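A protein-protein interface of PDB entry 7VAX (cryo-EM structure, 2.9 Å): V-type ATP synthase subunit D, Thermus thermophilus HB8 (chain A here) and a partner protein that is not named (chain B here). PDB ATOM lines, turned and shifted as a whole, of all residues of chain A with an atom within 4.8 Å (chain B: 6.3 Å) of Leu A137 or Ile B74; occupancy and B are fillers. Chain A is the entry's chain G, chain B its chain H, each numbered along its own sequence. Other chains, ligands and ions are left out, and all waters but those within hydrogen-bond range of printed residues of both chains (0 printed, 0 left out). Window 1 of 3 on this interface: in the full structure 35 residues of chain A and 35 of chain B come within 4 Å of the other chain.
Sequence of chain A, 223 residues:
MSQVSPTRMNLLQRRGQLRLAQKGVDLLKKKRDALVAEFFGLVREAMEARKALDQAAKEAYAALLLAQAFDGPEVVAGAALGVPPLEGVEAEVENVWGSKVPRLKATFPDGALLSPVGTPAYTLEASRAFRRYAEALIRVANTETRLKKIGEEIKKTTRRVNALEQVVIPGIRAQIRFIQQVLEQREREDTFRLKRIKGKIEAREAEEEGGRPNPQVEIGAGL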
ATOM      1  N   LEU A  53     -17.435 -13.019 -25.046  1.00  0.00           N
ATOM      2  CA  LEU A  53     -17.772 -11.681 -24.573  1.00  0.00           C
ATOM      3  C   LEU A  53     -18.193 -11.702 -23.110  1.00  0.00           C
ATOM      4  O   LEU A  53     -17.828 -10.808 -22.342  1.00  0.00           O
ATOM      5  CB  LEU A  53     -18.883 -11.087 -25.436  1.00  0.00           C
ATOM      6  CG  LEU A  53     -19.480  -9.769 -24.946  1.00  0.00           C
ATOM      7  CD1 LEU A  53     -18.549  -8.620 -25.278  1.00  0.00           C
ATOM      8  CD2 LEU A  53     -20.859  -9.539 -25.542  1.00  0.00           C
ATOM      9  N   TYR A 133     -12.441  -6.147 -23.534  1.00  0.00           N
ATOM     10  CA  TYR A 133     -13.895  -6.274 -23.526  1.00  0.00           C
ATOM     11  C   TYR A 133     -14.520  -5.543 -24.708  1.00  0.00           C
ATOM     12  O   TYR A 133     -15.463  -6.044 -25.329  1.00  0.00           O
ATOM     13  CB  TYR A 133     -14.444  -5.740 -22.203  1.00  0.00           C
ATOM     14  CG  TYR A 133     -15.946  -5.799 -22.072  1.00  0.00           C
ATOM     15  CD1 TYR A 133     -16.646  -6.956 -22.382  1.00  0.00           C
ATOM     16  CD2 TYR A 133     -16.664  -4.700 -21.623  1.00  0.00           C
ATOM     17  CE1 TYR A 133     -18.019  -7.010 -22.260  1.00  0.00           C
ATOM     18  CE2 TYR A 133     -18.038  -4.747 -21.496  1.00  0.00           C
ATOM     19  CZ  TYR A 133     -18.711  -5.905 -21.814  1.00  0.00           C
ATOM     20  OH  TYR A 133     -20.080  -5.959 -21.690  1.00  0.00           O
ATOM     21  N   ALA A 134     -14.011  -4.353 -25.030  1.00  0.00           N
ATOM     22  CA  ALA A 134     -14.509  -3.609 -26.183  1.00  0.00           C
ATOM     23  C   ALA A 134     -14.204  -4.339 -27.485  1.00  0.00           C
ATOM     24  O   ALA A 134     -15.023  -4.335 -28.412  1.00  0.00           O
ATOM     25  CB  ALA A 134     -13.910  -2.205 -26.200  1.00  0.00           C
ATOM     26  N   GLU A 135     -13.024  -4.956 -27.581  1.00  0.00           N
ATOM     27  CA  GLU A 135     -12.708  -5.761 -28.759  1.00  0.00           C
ATOM     28  C   GLU A 135     -13.689  -6.921 -28.903  1.00  0.00           C
ATOM     29  O   GLU A 135     -14.197  -7.196 -30.001  1.00  0.00           O
ATOM     30  CB  GLU A 135     -11.269  -6.275 -28.669  1.00  0.00           C
ATOM     31  CG  GLU A 135     -10.750  -6.925 -29.943  1.00  0.00           C
ATOM     32  CD  GLU A 135     -11.082  -8.403 -30.027  1.00  0.00           C
ATOM     33  OE1 GLU A 135     -11.094  -9.072 -28.972  1.00  0.00           O
ATOM     34  OE2 GLU A 135     -11.337  -8.894 -31.147  1.00  0.00           O
ATOM     35  N   ALA A 136     -13.976  -7.608 -27.796  1.00  0.00           N
ATOM     36  CA  ALA A 136     -14.953  -8.692 -27.838  1.00  0.00           C
ATOM     37  C   ALA A 136     -16.332  -8.172 -28.228  1.00  0.00           C
ATOM     38  O   ALA A 136     -17.071  -8.837 -28.963  1.00  0.00           O
ATOM     39  CB  ALA A 136     -15.007  -9.405 -26.488  1.00  0.00           C
ATOM     40  N   LEU A 137     -16.693  -6.983 -27.741  1.00  0.00           N
ATOM     41  CA  LEU A 137     -17.987  -6.400 -28.078  1.00  0.00           C
ATOM     42  C   LEU A 137     -18.094  -6.083 -29.564  1.00  0.00           C
ATOM     43  O   LEU A 137     -19.134  -6.334 -30.185  1.00  0.00           O
ATOM     44  CB  LEU A 137     -18.227  -5.141 -27.247  1.00  0.00           C
ATOM     45  CG  LEU A 137     -19.617  -4.537 -27.439  1.00  0.00           C
ATOM     46  CD1 LEU A 137     -20.669  -5.552 -27.045  1.00  0.00           C
ATOM     47  CD2 LEU A 137     -19.770  -3.255 -26.636  1.00  0.00           C
ATOM     48  N   ILE A 138     -17.039  -5.511 -30.151  1.00  0.00           N
ATOM     49  CA  ILE A 138     -17.109  -5.208 -31.577  1.00  0.00           C
ATOM     50  C   ILE A 138     -17.141  -6.498 -32.389  1.00  0.00           C
ATOM     51  O   ILE A 138     -17.826  -6.569 -33.415  1.00  0.00           O
ATOM     52  CB  ILE A 138     -15.967  -4.271 -32.025  1.00  0.00           C
ATOM     53  CG1 ILE A 138     -14.617  -4.987 -32.052  1.00  0.00           C
ATOM     54  CG2 ILE A 138     -15.917  -3.027 -31.147  1.00  0.00           C
ATOM     55  CD1 ILE A 138     -13.584  -4.310 -32.926  1.00  0.00           C
ATOM     56  N   ARG A 139     -16.437  -7.542 -31.939  1.00  0.00           N
ATOM     57  CA  ARG A 139     -16.546  -8.837 -32.609  1.00  0.00           C
ATOM     58  C   ARG A 139     -17.976  -9.370 -32.555  1.00  0.00           C
ATOM     59  O   ARG A 139     -18.514  -9.847 -33.565  1.00  0.00           O
ATOM     60  CB  ARG A 139     -15.580  -9.835 -31.975  1.00  0.00           C
ATOM     61  CG  ARG A 139     -15.672 -11.238 -32.549  1.00  0.00           C
ATOM     62  CD  ARG A 139     -14.895 -12.232 -31.703  1.00  0.00           C
ATOM     63  NE  ARG A 139     -15.127 -13.606 -32.128  1.00  0.00           N
ATOM     64  CZ  ARG A 139     -14.592 -14.671 -31.546  1.00  0.00           C
ATOM     65  NH1 ARG A 139     -13.779 -14.557 -30.509  1.00  0.00           N
ATOM     66  NH2 ARG A 139     -14.880 -15.881 -32.017  1.00  0.00           N
ATOM     67  N   VAL A 140     -18.608  -9.288 -31.383  1.00  0.00           N
ATOM     68  CA  VAL A 140     -19.970  -9.789 -31.225  1.00  0.00           C
ATOM     69  C   VAL A 140     -20.934  -9.011 -32.110  1.00  0.00           C
ATOM     70  O   VAL A 140     -21.809  -9.594 -32.760  1.00  0.00           O
ATOM     71  CB  VAL A 140     -20.389  -9.735 -29.743  1.00  0.00           C
ATOM     72  CG1 VAL A 140     -21.901  -9.769 -29.611  1.00  0.00           C
ATOM     73  CG2 VAL A 140     -19.760 -10.888 -28.979  1.00  0.00           C
ATOM     74  N   ALA A 141     -20.793  -7.685 -32.149  1.00  0.00           N
ATOM     75  CA  ALA A 141     -21.669  -6.874 -32.990  1.00  0.00           C
ATOM     76  C   ALA A 141     -21.455  -7.179 -34.467  1.00  0.00           C
ATOM     77  O   ALA A 141     -22.418  -7.235 -35.244  1.00  0.00           O
ATOM     78  CB  ALA A 141     -21.442  -5.391 -32.709  1.00  0.00           C
ATOM     79  N   ALA B   2     -20.434   3.927 -27.533  1.00  0.00           N
ATOM     80  CA  ALA B   2     -21.021   4.452 -26.310  1.00  0.00           C
ATOM     81  C   ALA B   2     -21.715   3.325 -25.561  1.00  0.00           C
ATOM     82  O   ALA B   2     -22.220   2.377 -26.167  1.00  0.00           O
ATOM     83  CB  ALA B   2     -22.009   5.585 -26.603  1.00  0.00           C
ATOM     84  N   VAL B   3     -21.730   3.441 -24.234  1.00  0.00           N
ATOM     85  CA  VAL B   3     -22.371   2.471 -23.354  1.00  0.00           C
ATOM     86  C   VAL B   3     -23.225   3.229 -22.347  1.00  0.00           C
ATOM     87  O   VAL B   3     -22.766   4.211 -21.754  1.00  0.00           O
ATOM     88  CB  VAL B   3     -21.341   1.581 -22.631  1.00  0.00           C
ATOM     89  CG1 VAL B   3     -22.045   0.603 -21.709  1.00  0.00           C
ATOM     90  CG2 VAL B   3     -20.486   0.832 -23.640  1.00  0.00           C
ATOM     91  N   ILE B   4     -24.461   2.773 -22.156  1.00  0.00           N
ATOM     92  CA  ILE B   4     -25.403   3.453 -21.274  1.00  0.00           C
ATOM     93  C   ILE B   4     -26.035   2.446 -20.316  1.00  0.00           C
ATOM     94  O   ILE B   4     -27.129   2.670 -19.783  1.00  0.00           O
ATOM     95  CB  ILE B   4     -26.456   4.219 -22.103  1.00  0.00           C
ATOM     96  CG1 ILE B   4     -27.116   5.326 -21.270  1.00  0.00           C
ATOM     97  CG2 ILE B   4     -27.469   3.266 -22.742  1.00  0.00           C
ATOM     98  CD1 ILE B   4     -27.858   6.353 -22.096  1.00  0.00           C
ATOM     99  N   ALA B   5     -25.336   1.335 -20.071  1.00  0.00           N
ATOM    100  CA  ALA B   5     -25.869   0.291 -19.201  1.00  0.00           C
ATOM    101  C   ALA B   5     -26.077   0.803 -17.778  1.00  0.00           C
ATOM    102  O   ALA B   5     -27.208   0.854 -17.281  1.00  0.00           O
ATOM    103  CB  ALA B   5     -24.937  -0.922 -19.210  1.00  0.00           C
ATOM    104  N   THR B   9     -20.387   0.567 -15.572  1.00  0.00           N
ATOM    105  CA  THR B   9     -19.907   0.259 -16.914  1.00  0.00           C
ATOM    106  C   THR B   9     -19.593   1.524 -17.701  1.00  0.00           C
ATOM    107  O   THR B   9     -18.664   1.530 -18.514  1.00  0.00           O
ATOM    108  CB  THR B   9     -20.934  -0.589 -17.665  1.00  0.00           C
ATOM    109  OG1 THR B   9     -21.314  -1.709 -16.855  1.00  0.00           O
ATOM    110  CG2 THR B   9     -20.357  -1.098 -18.973  1.00  0.00           C
ATOM    111  N   PHE B  13     -15.955   2.043 -19.340  1.00  0.00           N
ATOM    112  CA  PHE B  13     -15.732   2.321 -20.754  1.00  0.00           C
ATOM    113  C   PHE B  13     -15.088   3.685 -20.959  1.00  0.00           C
ATOM    114  O   PHE B  13     -14.298   3.860 -21.895  1.00  0.00           O
ATOM    115  CB  PHE B  13     -17.048   2.228 -21.522  1.00  0.00           C
ATOM    116  CG  PHE B  13     -17.326   0.862 -22.075  1.00  0.00           C
ATOM    117  CD1 PHE B  13     -17.947  -0.099 -21.299  1.00  0.00           C
ATOM    118  CD2 PHE B  13     -16.959   0.536 -23.369  1.00  0.00           C
ATOM    119  CE1 PHE B  13     -18.204  -1.358 -21.804  1.00  0.00           C
ATOM    120  CE2 PHE B  13     -17.212  -0.722 -23.880  1.00  0.00           C
ATOM    121  CZ  PHE B  13     -17.835  -1.671 -23.096  1.00  0.00           C
ATOM    122  N   LEU B  18     -14.141   4.871 -24.273  1.00  0.00           N
ATOM    123  CA  LEU B  18     -15.455   4.852 -24.910  1.00  0.00           C
ATOM    124  C   LEU B  18     -16.418   5.597 -23.999  1.00  0.00           C
ATOM    125  O   LEU B  18     -16.791   5.090 -22.937  1.00  0.00           O
ATOM    126  CB  LEU B  18     -15.930   3.422 -25.168  1.00  0.00           C
ATOM    127  CG  LEU B  18     -15.272   2.722 -26.359  1.00  0.00           C
ATOM    128  CD1 LEU B  18     -15.891   1.356 -26.602  1.00  0.00           C
ATOM    129  CD2 LEU B  18     -15.361   3.587 -27.607  1.00  0.00           C
ATOM    130  N   LEU B  44     -21.437   2.254 -32.685  1.00  0.00           N
ATOM    131  CA  LEU B  44     -22.036   1.285 -31.777  1.00  0.00           C
ATOM    132  C   LEU B  44     -22.596   1.969 -30.538  1.00  0.00           C
ATOM    133  O   LEU B  44     -22.030   2.948 -30.046  1.00  0.00           O
ATOM    134  CB  LEU B  44     -21.010   0.221 -31.364  1.00  0.00           C
ATOM    135  CG  LEU B  44     -21.506  -1.000 -30.585  1.00  0.00           C
ATOM    136  CD1 LEU B  44     -20.780  -2.244 -31.056  1.00  0.00           C
ATOM    137  CD2 LEU B  44     -21.314  -0.809 -29.088  1.00  0.00           C
ATOM    138  N   ALA B  46     -24.309   0.439 -26.775  1.00  0.00           N
ATOM    139  CA  ALA B  46     -24.478  -0.788 -26.005  1.00  0.00           C
ATOM    140  C   ALA B  46     -25.357  -0.534 -24.788  1.00  0.00           C
ATOM    141  O   ALA B  46     -25.159   0.451 -24.069  1.00  0.00           O
ATOM    142  CB  ALA B  46     -23.119  -1.343 -25.567  1.00  0.00           C
ATOM    143  N   VAL B  47     -26.327  -1.421 -24.560  1.00  0.00           N
ATOM    144  CA  VAL B  47     -27.228  -1.347 -23.412  1.00  0.00           C
ATOM    145  C   VAL B  47     -27.327  -2.723 -22.766  1.00  0.00           C
ATOM    146  O   VAL B  47     -27.354  -3.742 -23.463  1.00  0.00           O
ATOM    147  CB  VAL B  47     -28.634  -0.842 -23.810  1.00  0.00           C
ATOM    148  CG1 VAL B  47     -29.431  -0.459 -22.570  1.00  0.00           C
ATOM    149  CG2 VAL B  47     -28.540   0.340 -24.763  1.00  0.00           C
ATOM    150  N   ASP B  48     -27.377  -2.752 -21.435  1.00  0.00           N
ATOM    151  CA  ASP B  48     -27.621  -3.995 -20.714  1.00  0.00           C
ATOM    152  C   ASP B  48     -29.041  -4.495 -20.968  1.00  0.00           C
ATOM    153  O   ASP B  48     -29.948  -3.723 -21.292  1.00  0.00           O
ATOM    154  CB  ASP B  48     -27.402  -3.803 -19.215  1.00  0.00           C
ATOM    155  CG  ASP B  48     -28.125  -2.587 -18.671  1.00  0.00           C
ATOM    156  OD1 ASP B  48     -28.576  -1.747 -19.481  1.00  0.00           O
ATOM    157  OD2 ASP B  48     -28.243  -2.468 -17.433  1.00  0.00           O
ATOM    158  N   GLU B  49     -29.227  -5.812 -20.826  1.00  0.00           N
ATOM    159  CA  GLU B  49     -30.520  -6.413 -21.138  1.00  0.00           C
ATOM    160  C   GLU B  49     -31.597  -6.019 -20.136  1.00  0.00           C
ATOM    161  O   GLU B  49     -32.778  -5.980 -20.499  1.00  0.00           O
ATOM    162  CB  GLU B  49     -30.418  -7.942 -21.175  1.00  0.00           C
ATOM    163  CG  GLU B  49     -30.191  -8.620 -19.828  1.00  0.00           C
ATOM    164  CD  GLU B  49     -28.735  -8.664 -19.423  1.00  0.00           C
ATOM    165  OE1 GLU B  49     -27.947  -7.909 -20.025  1.00  0.00           O
ATOM    166  OE2 GLU B  49     -28.374  -9.455 -18.524  1.00  0.00           O
ATOM    167  N   ALA B  50     -31.222  -5.738 -18.886  1.00  0.00           N
ATOM    168  CA  ALA B  50     -32.221  -5.434 -17.867  1.00  0.00           C
ATOM    169  C   ALA B  50     -32.918  -4.115 -18.166  1.00  0.00           C
ATOM    170  O   ALA B  50     -34.142  -4.001 -18.030  1.00  0.00           O
ATOM    171  CB  ALA B  50     -31.574  -5.403 -16.482  1.00  0.00           C
ATOM    172  N   LEU B  72     -27.107  -3.328 -29.583  1.00  0.00           N
ATOM    173  CA  LEU B  72     -27.032  -4.709 -29.140  1.00  0.00           C
ATOM    174  C   LEU B  72     -27.030  -4.768 -27.623  1.00  0.00           C
ATOM    175  O   LEU B  72     -26.463  -3.872 -26.975  1.00  0.00           O
ATOM    176  CB  LEU B  72     -25.781  -5.415 -29.682  1.00  0.00           C
ATOM    177  CG  LEU B  72     -24.422  -5.138 -29.034  1.00  0.00           C
ATOM    178  CD1 LEU B  72     -23.407  -6.178 -29.486  1.00  0.00           C
ATOM    179  CD2 LEU B  72     -23.916  -3.736 -29.332  1.00  0.00           C
ATOM    180  N   PRO B  73     -27.652  -5.784 -27.029  1.00  0.00           N
ATOM    181  CA  PRO B  73     -27.570  -5.951 -25.573  1.00  0.00           C
ATOM    182  C   PRO B  73     -26.167  -6.349 -25.139  1.00  0.00           C
ATOM    183  O   PRO B  73     -25.405  -6.957 -25.895  1.00  0.00           O
ATOM    184  CB  PRO B  73     -28.579  -7.070 -25.287  1.00  0.00           C
ATOM    185  CG  PRO B  73     -29.455  -7.124 -26.496  1.00  0.00           C
ATOM    186  CD  PRO B  73     -28.570  -6.754 -27.642  1.00  0.00           C
ATOM    187  N   ILE B  74     -25.828  -5.989 -23.905  1.00  0.00           N
ATOM    188  CA  ILE B  74     -24.559  -6.339 -23.282  1.00  0.00           C
ATOM    189  C   ILE B  74     -24.837  -6.827 -21.866  1.00  0.00           C
ATOM    190  O   ILE B  74     -25.989  -6.953 -21.451  1.00  0.00           O
ATOM    191  CB  ILE B  74     -23.560  -5.160 -23.280  1.00  0.00           C
ATOM    192  CG1 ILE B  74     -24.135  -3.953 -22.535  1.00  0.00           C
ATOM    193  CG2 ILE B  74     -23.155  -4.811 -24.696  1.00  0.00           C
ATOM    194  CD1 ILE B  74     -23.103  -2.889 -22.217  1.00  0.00           C
ATOM    195  N   ALA B  75     -23.768  -7.119 -21.130  1.00  0.00           N
ATOM    196  CA  ALA B  75     -23.881  -7.596 -19.763  1.00  0.00           C
ATOM    197  C   ALA B  75     -23.612  -6.458 -18.787  1.00  0.00           C
ATOM    198  O   ALA B  75     -22.649  -5.705 -18.949  1.00  0.00           O
ATOM    199  CB  ALA B  75     -22.918  -8.756 -19.496  1.00  0.00           C
ATOM    200  N   GLY B  76     -24.476  -6.331 -17.781  1.00  0.00           N
ATOM    201  CA  GLY B  76     -24.360  -5.281 -16.790  1.00  0.00           C
ATOM    202  C   GLY B  76     -23.383  -5.636 -15.686  1.00  0.00           C
ATOM    203  O   GLY B  76     -22.654  -6.630 -15.740  1.00  0.00           O
ATOM    204  N   GLU B  79     -25.284  -8.896 -13.435  1.00  0.00           N
ATOM    205  CA  GLU B  79     -25.683 -10.072 -14.197  1.00  0.00           C
ATOM    206  C   GLU B  79     -24.516 -10.702 -14.945  1.00  0.00           C
ATOM    207  O   GLU B  79     -24.591 -11.885 -15.300  1.00  0.00           O
ATOM    208  CB  GLU B  79     -26.805  -9.713 -15.171  1.00  0.00           C
ATOM    209  CG  GLU B  79     -26.468  -8.587 -16.132  1.00  0.00           C
ATOM    210  CD  GLU B  79     -26.867  -7.224 -15.601  1.00  0.00           C
ATOM    211  OE1 GLU B  79     -26.359  -6.830 -14.531  1.00  0.00           O
ATOM    212  OE2 GLU B  79     -27.691  -6.549 -16.254  1.00  0.00           O
ATOM    213  N   HIS B  84     -24.691 -14.610 -17.837  1.00  0.00           N
ATOM    214  CA  HIS B  84     -25.673 -14.320 -18.872  1.00  0.00           C
ATOM    215  C   HIS B  84     -26.079 -15.596 -19.598  1.00  0.00           C
ATOM    216  O   HIS B  84     -25.253 -16.476 -19.857  1.00  0.00           O
ATOM    217  CB  HIS B  84     -25.112 -13.304 -19.865  1.00  0.00           C
ATOM    218  CG  HIS B  84     -26.118 -12.807 -20.856  1.00  0.00           C
ATOM    219  ND1 HIS B  84     -27.407 -12.472 -20.501  1.00  0.00           N
ATOM    220  CD2 HIS B  84     -26.025 -12.585 -22.188  1.00  0.00           C
ATOM    221  CE1 HIS B  84     -28.064 -12.066 -21.573  1.00  0.00           C
ATOM    222  NE2 HIS B  84     -27.248 -12.125 -22.609  1.00  0.00           N
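The backbone carbonyl oxygen of Leu B44 is in hydrogen-bond range of the backbone NH of Ala B2, at 3.1 Å. O of Phe B13 sits at hydrogen-bond distance from N of Leu B18 (2.6 Å). The backbone NH (N) of Val B47 sits at hydrogen-bond distance from the backbone carbonyl oxygen (O) of Leu B72, 3.4 Å away. The backbone NH (N) of Ile B74 lies within hydrogen-bond range of the backbone carbonyl oxygen (O) of Val B47 (2.8 Å). O of Ile B74 sits at hydrogen-bond distance from N of Glu B49, 3.5 Å away.
Among the printed residues, merely in contact across the chains: Tyr A133 with Phe B13, Leu A137 with Ile B74, Ala A141 with Leu B44, Leu A137 with Leu B72, Tyr A133 with Ala B75, Leu A137 with Leu B44, Ala A141 with Leu B72, Val A140 with Leu B72 and Tyr A133 with Ile B74.
Printed residues of chain B within 4 Å of Leu A137: Leu B44 (3.8 Å), Leu B72 (3.7 Å) and Ile B74 (3.5 Å). Of chain A, only Tyr A133 and Leu A137 come within 4 Å of Ile B74. Of the printed residues of chain A, Phe B13 touches Tyr A133. Printed residues of chain A within 4 Å of Leu B44: Leu A137 and Ala A141. The nearest printed residue of chain A that does not touch Leu B44 is Ile A138 (4.7 Å).
Hydrophobic or aromatic side chains of chain B within 4 Å of the printed part of chain A: Phe B13, Leu B44, Leu B72 and Ile B74. Hydrophobic or aromatic side chains of chain A within 4 Å of the printed part of chain B: Tyr A133, Leu A137, Val A140 and Ala A141. Among the printed residues, 9 pairs touch across the chains. Among the printed residues, no Asp or Glu carboxylate lies within 4 Å of a Lys or Arg side-chain nitrogen of the other chain.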
